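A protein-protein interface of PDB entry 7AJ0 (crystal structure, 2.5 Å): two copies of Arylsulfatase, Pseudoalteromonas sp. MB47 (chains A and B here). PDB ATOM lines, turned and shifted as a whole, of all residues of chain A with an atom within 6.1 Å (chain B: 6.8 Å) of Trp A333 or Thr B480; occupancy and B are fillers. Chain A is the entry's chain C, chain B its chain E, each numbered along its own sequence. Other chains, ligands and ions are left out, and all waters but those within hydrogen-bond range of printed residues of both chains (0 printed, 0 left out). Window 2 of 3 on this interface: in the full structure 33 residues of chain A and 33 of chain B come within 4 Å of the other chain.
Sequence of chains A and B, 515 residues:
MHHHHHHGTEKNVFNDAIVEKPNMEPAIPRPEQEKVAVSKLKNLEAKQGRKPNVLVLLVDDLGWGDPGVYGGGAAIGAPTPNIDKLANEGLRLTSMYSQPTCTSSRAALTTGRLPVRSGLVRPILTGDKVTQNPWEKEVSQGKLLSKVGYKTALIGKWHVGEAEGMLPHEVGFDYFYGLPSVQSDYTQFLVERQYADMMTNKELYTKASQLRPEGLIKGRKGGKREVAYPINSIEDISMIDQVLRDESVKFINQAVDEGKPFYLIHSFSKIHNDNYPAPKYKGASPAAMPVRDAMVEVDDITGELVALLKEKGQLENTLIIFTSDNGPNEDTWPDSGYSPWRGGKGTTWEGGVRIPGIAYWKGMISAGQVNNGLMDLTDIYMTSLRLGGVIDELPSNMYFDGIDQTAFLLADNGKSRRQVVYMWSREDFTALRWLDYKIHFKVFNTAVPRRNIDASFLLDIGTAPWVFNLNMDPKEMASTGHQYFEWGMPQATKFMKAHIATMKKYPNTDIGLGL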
ATOM      1  N   ASN A 329     -14.817 -22.422  -9.643  1.00  0.00           N
ATOM      2  CA  ASN A 329     -15.912 -21.526 -10.008  1.00  0.00           C
ATOM      3  C   ASN A 329     -16.170 -21.681 -11.501  1.00  0.00           C
ATOM      4  O   ASN A 329     -15.616 -20.958 -12.332  1.00  0.00           O
ATOM      5  CB  ASN A 329     -15.581 -20.082  -9.649  1.00  0.00           C
ATOM      6  CG  ASN A 329     -16.763 -19.151  -9.838  1.00  0.00           C
ATOM      7  OD1 ASN A 329     -17.765 -19.518 -10.452  1.00  0.00           O
ATOM      8  ND2 ASN A 329     -16.651 -17.936  -9.312  1.00  0.00           N
ATOM      9  N   GLU A 330     -17.030 -22.640 -11.849  1.00  0.00           N
ATOM     10  CA  GLU A 330     -17.367 -22.863 -13.247  1.00  0.00           C
ATOM     11  C   GLU A 330     -18.154 -21.704 -13.846  1.00  0.00           C
ATOM     12  O   GLU A 330     -18.168 -21.550 -15.071  1.00  0.00           O
ATOM     13  CB  GLU A 330     -18.166 -24.161 -13.389  1.00  0.00           C
ATOM     14  CG  GLU A 330     -17.451 -25.391 -12.857  1.00  0.00           C
ATOM     15  CD  GLU A 330     -18.134 -26.688 -13.255  1.00  0.00           C
ATOM     16  OE1 GLU A 330     -19.380 -26.708 -13.347  1.00  0.00           O
ATOM     17  OE2 GLU A 330     -17.419 -27.688 -13.485  1.00  0.00           O
ATOM     18  N   ASP A 331     -18.797 -20.882 -13.014  1.00  0.00           N
ATOM     19  CA  ASP A 331     -19.617 -19.795 -13.536  1.00  0.00           C
ATOM     20  C   ASP A 331     -18.786 -18.767 -14.294  1.00  0.00           C
ATOM     21  O   ASP A 331     -19.316 -18.069 -15.167  1.00  0.00           O
ATOM     22  CB  ASP A 331     -20.374 -19.110 -12.396  1.00  0.00           C
ATOM     23  CG  ASP A 331     -21.423 -20.006 -11.772  1.00  0.00           C
ATOM     24  OD1 ASP A 331     -21.046 -20.982 -11.090  1.00  0.00           O
ATOM     25  OD2 ASP A 331     -22.627 -19.731 -11.966  1.00  0.00           O
ATOM     26  N   THR A 332     -17.497 -18.646 -13.967  1.00  0.00           N
ATOM     27  CA  THR A 332     -16.603 -17.700 -14.624  1.00  0.00           C
ATOM     28  C   THR A 332     -15.724 -18.372 -15.675  1.00  0.00           C
ATOM     29  O   THR A 332     -14.624 -17.893 -15.971  1.00  0.00           O
ATOM     30  CB  THR A 332     -15.735 -16.976 -13.590  1.00  0.00           C
ATOM     31  OG1 THR A 332     -15.016 -17.929 -12.795  1.00  0.00           O
ATOM     32  CG2 THR A 332     -16.596 -16.108 -12.681  1.00  0.00           C
ATOM     33  N   TRP A 333     -16.191 -19.478 -16.243  1.00  0.00           N
ATOM     34  CA  TRP A 333     -15.448 -20.144 -17.304  1.00  0.00           C
ATOM     35  C   TRP A 333     -15.204 -19.166 -18.450  1.00  0.00           C
ATOM     36  O   TRP A 333     -16.081 -18.355 -18.767  1.00  0.00           O
ATOM     37  CB  TRP A 333     -16.227 -21.365 -17.795  1.00  0.00           C
ATOM     38  CG  TRP A 333     -15.442 -22.251 -18.701  1.00  0.00           C
ATOM     39  CD1 TRP A 333     -14.689 -23.331 -18.344  1.00  0.00           C
ATOM     40  CD2 TRP A 333     -15.319 -22.128 -20.122  1.00  0.00           C
ATOM     41  NE1 TRP A 333     -14.104 -23.889 -19.454  1.00  0.00           N
ATOM     42  CE2 TRP A 333     -14.475 -23.169 -20.559  1.00  0.00           C
ATOM     43  CE3 TRP A 333     -15.837 -21.239 -21.066  1.00  0.00           C
ATOM     44  CZ2 TRP A 333     -14.145 -23.347 -21.898  1.00  0.00           C
ATOM     45  CZ3 TRP A 333     -15.507 -21.417 -22.394  1.00  0.00           C
ATOM     46  CH2 TRP A 333     -14.670 -22.463 -22.799  1.00  0.00           C
ATOM     47  N   PRO A 334     -14.030 -19.207 -19.103  1.00  0.00           N
ATOM     48  CA  PRO A 334     -12.889 -20.116 -18.934  1.00  0.00           C
ATOM     49  C   PRO A 334     -11.885 -19.685 -17.867  1.00  0.00           C
ATOM     50  O   PRO A 334     -10.756 -20.174 -17.850  1.00  0.00           O
ATOM     51  CB  PRO A 334     -12.229 -20.087 -20.321  1.00  0.00           C
ATOM     52  CG  PRO A 334     -12.478 -18.688 -20.796  1.00  0.00           C
ATOM     53  CD  PRO A 334     -13.821 -18.272 -20.226  1.00  0.00           C
ATOM     54  N   ASP A 335     -12.292 -18.780 -16.983  1.00  0.00           N
ATOM     55  CA  ASP A 335     -11.446 -18.361 -15.866  1.00  0.00           C
ATOM     56  C   ASP A 335     -11.755 -19.216 -14.633  1.00  0.00           C
ATOM     57  O   ASP A 335     -12.075 -18.721 -13.553  1.00  0.00           O
ATOM     58  CB  ASP A 335     -11.647 -16.876 -15.590  1.00  0.00           C
ATOM     59  CG  ASP A 335     -10.473 -16.251 -14.865  1.00  0.00           C
ATOM     60  OD1 ASP A 335      -9.544 -16.992 -14.476  1.00  0.00           O
ATOM     61  OD2 ASP A 335     -10.478 -15.013 -14.689  1.00  0.00           O
ATOM     62  N   SER A 336     -11.647 -20.532 -14.820  1.00  0.00           N
ATOM     63  CA  SER A 336     -12.068 -21.490 -13.811  1.00  0.00           C
ATOM     64  C   SER A 336     -11.032 -22.594 -13.658  1.00  0.00           C
ATOM     65  O   SER A 336     -10.306 -22.924 -14.599  1.00  0.00           O
ATOM     66  CB  SER A 336     -13.418 -22.140 -14.170  1.00  0.00           C
ATOM     67  OG  SER A 336     -14.355 -21.188 -14.638  1.00  0.00           O
ATOM     68  N   ARG A 450     -22.514 -25.292 -16.323  1.00  0.00           N
ATOM     69  CA  ARG A 450     -21.451 -24.600 -15.608  1.00  0.00           C
ATOM     70  C   ARG A 450     -21.988 -23.589 -14.592  1.00  0.00           C
ATOM     71  O   ARG A 450     -21.210 -23.093 -13.775  1.00  0.00           O
ATOM     72  CB  ARG A 450     -20.474 -23.858 -16.541  1.00  0.00           C
ATOM     73  CG  ARG A 450     -19.687 -24.736 -17.500  1.00  0.00           C
ATOM     74  CD  ARG A 450     -18.538 -23.937 -18.118  1.00  0.00           C
ATOM     75  NE  ARG A 450     -17.823 -24.677 -19.153  1.00  0.00           N
ATOM     76  CZ  ARG A 450     -17.934 -24.446 -20.460  1.00  0.00           C
ATOM     77  NH1 ARG A 450     -18.729 -23.484 -20.916  1.00  0.00           N
ATOM     78  NH2 ARG A 450     -17.238 -25.181 -21.315  1.00  0.00           N
ATOM     79  N   PRO B 465     -18.887 -27.388 -36.458  1.00  0.00           N
ATOM     80  CA  PRO B 465     -18.462 -28.519 -35.625  1.00  0.00           C
ATOM     81  C   PRO B 465     -18.304 -28.082 -34.178  1.00  0.00           C
ATOM     82  O   PRO B 465     -18.004 -26.922 -33.885  1.00  0.00           O
ATOM     83  CB  PRO B 465     -17.119 -28.937 -36.237  1.00  0.00           C
ATOM     84  CG  PRO B 465     -17.124 -28.371 -37.619  1.00  0.00           C
ATOM     85  CD  PRO B 465     -17.931 -27.109 -37.547  1.00  0.00           C
ATOM     86  N   TRP B 466     -18.515 -29.024 -33.265  1.00  0.00           N
ATOM     87  CA  TRP B 466     -18.349 -28.744 -31.847  1.00  0.00           C
ATOM     88  C   TRP B 466     -16.863 -28.709 -31.512  1.00  0.00           C
ATOM     89  O   TRP B 466     -16.110 -29.610 -31.898  1.00  0.00           O
ATOM     90  CB  TRP B 466     -19.057 -29.796 -31.000  1.00  0.00           C
ATOM     91  CG  TRP B 466     -20.550 -29.753 -31.088  1.00  0.00           C
ATOM     92  CD1 TRP B 466     -21.302 -29.278 -32.121  1.00  0.00           C
ATOM     93  CD2 TRP B 466     -21.476 -30.202 -30.092  1.00  0.00           C
ATOM     94  NE1 TRP B 466     -22.638 -29.406 -31.833  1.00  0.00           N
ATOM     95  CE2 TRP B 466     -22.771 -29.971 -30.593  1.00  0.00           C
ATOM     96  CE3 TRP B 466     -21.335 -30.778 -28.825  1.00  0.00           C
ATOM     97  CZ2 TRP B 466     -23.919 -30.295 -29.871  1.00  0.00           C
ATOM     98  CZ3 TRP B 466     -22.475 -31.099 -28.112  1.00  0.00           C
ATOM     99  CH2 TRP B 466     -23.750 -30.858 -28.635  1.00  0.00           C
ATOM    100  N   VAL B 467     -16.439 -27.671 -30.800  1.00  0.00           N
ATOM    101  CA  VAL B 467     -15.035 -27.474 -30.462  1.00  0.00           C
ATOM    102  C   VAL B 467     -14.908 -27.336 -28.954  1.00  0.00           C
ATOM    103  O   VAL B 467     -15.689 -26.615 -28.320  1.00  0.00           O
ATOM    104  CB  VAL B 467     -14.447 -26.244 -31.171  1.00  0.00           C
ATOM    105  CG1 VAL B 467     -13.006 -26.023 -30.733  1.00  0.00           C
ATOM    106  CG2 VAL B 467     -14.526 -26.415 -32.669  1.00  0.00           C
ATOM    107  N   PHE B 468     -13.923 -28.027 -28.391  1.00  0.00           N
ATOM    108  CA  PHE B 468     -13.571 -27.898 -26.987  1.00  0.00           C
ATOM    109  C   PHE B 468     -12.068 -27.694 -26.888  1.00  0.00           C
ATOM    110  O   PHE B 468     -11.296 -28.475 -27.455  1.00  0.00           O
ATOM    111  CB  PHE B 468     -13.958 -29.140 -26.180  1.00  0.00           C
ATOM    112  CG  PHE B 468     -15.410 -29.497 -26.263  1.00  0.00           C
ATOM    113  CD1 PHE B 468     -15.871 -30.340 -27.256  1.00  0.00           C
ATOM    114  CD2 PHE B 468     -16.310 -29.008 -25.334  1.00  0.00           C
ATOM    115  CE1 PHE B 468     -17.206 -30.679 -27.331  1.00  0.00           C
ATOM    116  CE2 PHE B 468     -17.645 -29.346 -25.401  1.00  0.00           C
ATOM    117  CZ  PHE B 468     -18.094 -30.182 -26.401  1.00  0.00           C
ATOM    118  N   ASN B 469     -11.652 -26.651 -26.179  1.00  0.00           N
ATOM    119  CA  ASN B 469     -10.276 -26.567 -25.708  1.00  0.00           C
ATOM    120  C   ASN B 469     -10.162 -27.511 -24.515  1.00  0.00           C
ATOM    121  O   ASN B 469     -10.678 -27.216 -23.430  1.00  0.00           O
ATOM    122  CB  ASN B 469      -9.907 -25.138 -25.336  1.00  0.00           C
ATOM    123  CG  ASN B 469      -8.444 -24.996 -24.957  1.00  0.00           C
ATOM    124  OD1 ASN B 469      -7.837 -25.919 -24.412  1.00  0.00           O
ATOM    125  ND2 ASN B 469      -7.872 -23.835 -25.241  1.00  0.00           N
ATOM    126  N   MET B 472      -8.975 -26.226 -21.207  1.00  0.00           N
ATOM    127  CA  MET B 472      -9.916 -25.390 -20.479  1.00  0.00           C
ATOM    128  C   MET B 472     -11.247 -26.078 -20.215  1.00  0.00           C
ATOM    129  O   MET B 472     -11.958 -25.680 -19.284  1.00  0.00           O
ATOM    130  CB  MET B 472     -10.162 -24.091 -21.254  1.00  0.00           C
ATOM    131  CG  MET B 472      -8.882 -23.354 -21.626  1.00  0.00           C
ATOM    132  SD  MET B 472      -7.739 -23.205 -20.236  1.00  0.00           S
ATOM    133  CE  MET B 472      -8.744 -22.277 -19.085  1.00  0.00           C
ATOM    134  N   ASP B 473     -11.599 -27.093 -20.999  1.00  0.00           N
ATOM    135  CA  ASP B 473     -12.866 -27.812 -20.847  1.00  0.00           C
ATOM    136  C   ASP B 473     -12.598 -29.297 -21.042  1.00  0.00           C
ATOM    137  O   ASP B 473     -13.072 -29.915 -22.002  1.00  0.00           O
ATOM    138  CB  ASP B 473     -13.907 -27.294 -21.842  1.00  0.00           C
ATOM    139  CG  ASP B 473     -15.308 -27.798 -21.541  1.00  0.00           C
ATOM    140  OD1 ASP B 473     -15.487 -28.499 -20.521  1.00  0.00           O
ATOM    141  OD2 ASP B 473     -16.231 -27.487 -22.327  1.00  0.00           O
ATOM    142  N   PRO B 474     -11.828 -29.907 -20.137  1.00  0.00           N
ATOM    143  CA  PRO B 474     -11.486 -31.330 -20.306  1.00  0.00           C
ATOM    144  C   PRO B 474     -12.678 -32.263 -20.192  1.00  0.00           C
ATOM    145  O   PRO B 474     -12.621 -33.381 -20.718  1.00  0.00           O
ATOM    146  CB  PRO B 474     -10.468 -31.586 -19.183  1.00  0.00           C
ATOM    147  CG  PRO B 474     -10.788 -30.555 -18.146  1.00  0.00           C
ATOM    148  CD  PRO B 474     -11.251 -29.335 -18.904  1.00  0.00           C
ATOM    149  N   ALA B 478     -19.476 -27.883 -22.556  1.00  0.00           N
ATOM    150  CA  ALA B 478     -20.213 -26.955 -23.410  1.00  0.00           C
ATOM    151  C   ALA B 478     -19.313 -26.478 -24.536  1.00  0.00           C
ATOM    152  O   ALA B 478     -18.308 -25.804 -24.282  1.00  0.00           O
ATOM    153  CB  ALA B 478     -20.734 -25.766 -22.598  1.00  0.00           C
ATOM    154  N   SER B 479     -19.689 -26.802 -25.770  1.00  0.00           N
ATOM    155  CA  SER B 479     -18.878 -26.446 -26.924  1.00  0.00           C
ATOM    156  C   SER B 479     -18.910 -24.946 -27.186  1.00  0.00           C
ATOM    157  O   SER B 479     -19.946 -24.292 -27.045  1.00  0.00           O
ATOM    158  CB  SER B 479     -19.379 -27.196 -28.160  1.00  0.00           C
ATOM    159  OG  SER B 479     -18.943 -26.562 -29.350  1.00  0.00           O
ATOM    160  N   THR B 480     -17.753 -24.401 -27.571  1.00  0.00           N
ATOM    161  CA  THR B 480     -17.647 -23.020 -28.017  1.00  0.00           C
ATOM    162  C   THR B 480     -17.559 -22.901 -29.533  1.00  0.00           C
ATOM    163  O   THR B 480     -17.575 -21.780 -30.054  1.00  0.00           O
ATOM    164  CB  THR B 480     -16.421 -22.339 -27.386  1.00  0.00           C
ATOM    165  OG1 THR B 480     -15.257 -23.151 -27.577  1.00  0.00           O
ATOM    166  CG2 THR B 480     -16.638 -22.109 -25.896  1.00  0.00           C
ATOM    167  N   GLY B 481     -17.468 -24.023 -30.243  1.00  0.00           N
ATOM    168  CA  GLY B 481     -17.440 -23.985 -31.694  1.00  0.00           C
ATOM    169  C   GLY B 481     -16.387 -23.038 -32.228  1.00  0.00           C
ATOM    170  O   GLY B 481     -15.228 -23.043 -31.792  1.00  0.00           O
ATOM    171  N   HIS B 482     -16.799 -22.201 -33.180  1.00  0.00           N
ATOM    172  CA  HIS B 482     -15.898 -21.300 -33.882  1.00  0.00           C
ATOM    173  C   HIS B 482     -15.514 -20.069 -33.071  1.00  0.00           C
ATOM    174  O   HIS B 482     -14.626 -19.324 -33.499  1.00  0.00           O
ATOM    175  CB  HIS B 482     -16.554 -20.841 -35.193  1.00  0.00           C
ATOM    176  CG  HIS B 482     -17.558 -19.742 -35.010  1.00  0.00           C
ATOM    177  ND1 HIS B 482     -18.608 -19.831 -34.123  1.00  0.00           N
ATOM    178  CD2 HIS B 482     -17.661 -18.524 -35.593  1.00  0.00           C
ATOM    179  CE1 HIS B 482     -19.316 -18.716 -34.166  1.00  0.00           C
ATOM    180  NE2 HIS B 482     -18.764 -17.907 -35.051  1.00  0.00           N
ATOM    181  N   GLN B 483     -16.142 -19.845 -31.913  1.00  0.00           N
ATOM    182  CA  GLN B 483     -16.042 -18.550 -31.246  1.00  0.00           C
ATOM    183  C   GLN B 483     -14.592 -18.144 -31.004  1.00  0.00           C
ATOM    184  O   GLN B 483     -14.197 -17.008 -31.296  1.00  0.00           O
ATOM    185  CB  GLN B 483     -16.810 -18.583 -29.923  1.00  0.00           C
ATOM    186  CG  GLN B 483     -17.171 -17.207 -29.389  1.00  0.00           C
ATOM    187  CD  GLN B 483     -17.697 -17.250 -27.966  1.00  0.00           C
ATOM    188  OE1 GLN B 483     -17.802 -18.318 -27.364  1.00  0.00           O
ATOM    189  NE2 GLN B 483     -18.026 -16.084 -27.420  1.00  0.00           N
ATOM    190  N   TYR B 484     -13.786 -19.058 -30.462  1.00  0.00           N
ATOM    191  CA  TYR B 484     -12.395 -18.774 -30.137  1.00  0.00           C
ATOM    192  C   TYR B 484     -11.422 -19.534 -31.033  1.00  0.00           C
ATOM    193  O   TYR B 484     -10.253 -19.703 -30.674  1.00  0.00           O
ATOM    194  CB  TYR B 484     -12.108 -19.114 -28.672  1.00  0.00           C
ATOM    195  CG  TYR B 484     -13.019 -18.440 -27.674  1.00  0.00           C
ATOM    196  CD1 TYR B 484     -12.917 -17.079 -27.422  1.00  0.00           C
ATOM    197  CD2 TYR B 484     -13.969 -19.168 -26.968  1.00  0.00           C
ATOM    198  CE1 TYR B 484     -13.744 -16.457 -26.505  1.00  0.00           C
ATOM    199  CE2 TYR B 484     -14.801 -18.556 -26.049  1.00  0.00           C
ATOM    200  CZ  TYR B 484     -14.683 -17.201 -25.820  1.00  0.00           C
ATOM    201  OH  TYR B 484     -15.506 -16.585 -24.903  1.00  0.00           O
ATOM    202  N   PHE B 485     -11.886 -19.999 -32.203  1.00  0.00           N
ATOM    203  CA  PHE B 485     -11.085 -20.913 -33.016  1.00  0.00           C
ATOM    204  C   PHE B 485     -11.292 -20.669 -34.505  1.00  0.00           C
ATOM    205  O   PHE B 485     -11.173 -21.606 -35.302  1.00  0.00           O
ATOM    206  CB  PHE B 485     -11.438 -22.367 -32.641  1.00  0.00           C
ATOM    207  CG  PHE B 485     -10.387 -23.372 -33.015  1.00  0.00           C
ATOM    208  CD1 PHE B 485      -9.081 -23.239 -32.573  1.00  0.00           C
ATOM    209  CD2 PHE B 485     -10.717 -24.474 -33.786  1.00  0.00           C
ATOM    210  CE1 PHE B 485      -8.124 -24.174 -32.915  1.00  0.00           C
ATOM    211  CE2 PHE B 485      -9.767 -25.410 -34.128  1.00  0.00           C
ATOM    212  CZ  PHE B 485      -8.470 -25.264 -33.694  1.00  0.00           C
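Of the printed residues of chain B, Trp A333 touches Met B472, Asp B473 and Thr B480.
Of the printed residues of chain A, Thr B480 touches Trp A333 (3.7 Å).
Printed residues of chain A within 4 Å of Ala B478: Arg A450 (3.2 Å).
Of the printed residues of chain B, Pro A334 touches Met B472.
Printed residues of chain A within 4 Å of Asp B473: Trp A333 (3.95 Å) and Arg A450 (2.7 Å).
Of the printed residues of chain B, Arg A450 touches Asp B473 and Ala B478.
The nearest residue of chain B that does not touch Trp A333 is Tyr B484 (4.7 Å).
The nearest residue of chain A that does not touch Thr B480 is Arg A450 (5.5 Å).
The backbone NH (N) of Thr B480 lies within hydrogen-bond range of the backbone carbonyl oxygen (O) of Val B467, 3.1 Å away.
The backbone NH (N) of Ala B478 is in hydrogen-bond range of the side-chain carboxylate (OD2) of Asp B473, at 3.3 Å.
The side-chain hydroxyl (OG) of Ser A336 sits at hydrogen-bond distance from the backbone NH (N) of Trp A333 (3.0 Å).
OD1 of Asn B469 is in hydrogen-bond range of N of Met B472.
N of Asp A331 is in hydrogen-bond range of O of Arg A450 (3.4 Å).
NH2 of Arg A450 sits at hydrogen-bond distance from O of Ala B478, 3.2 Å away.
NH2 of Arg A450 lies within salt-bridge range of OD2 of Asp B473.
The indole nitrogen of Trp A333 is in hydrogen-bond range of the backbone carbonyl oxygen of Met B472 (2.8 Å).
No position is printed for both chains.
Of the 16 printed residues of chain B, 4 touch a printed residue of chain A.
Hydrophobic or aromatic side chains of chain B that line the printed part of chain A: Met B472 and Ala B478.
Along chain B the printed residues that touch a printed residue of chain A span positions 472 to 480.
Among the printed residues, 6 pairs touch across the chains.
Among the printed residues, Asp or Glu carboxylates within 4 Å of a Lys or Arg side-chain nitrogen of the other chain: Arg A450 with Asp B473 (2.7 Å).
Among the printed residues, pairs that only touch across the chains: Trp A333 with Asp B473 (3.95 Å), Trp A333 with Thr B480 (3.7 Å) and Pro A334 with Met B472 (3.2 Å).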
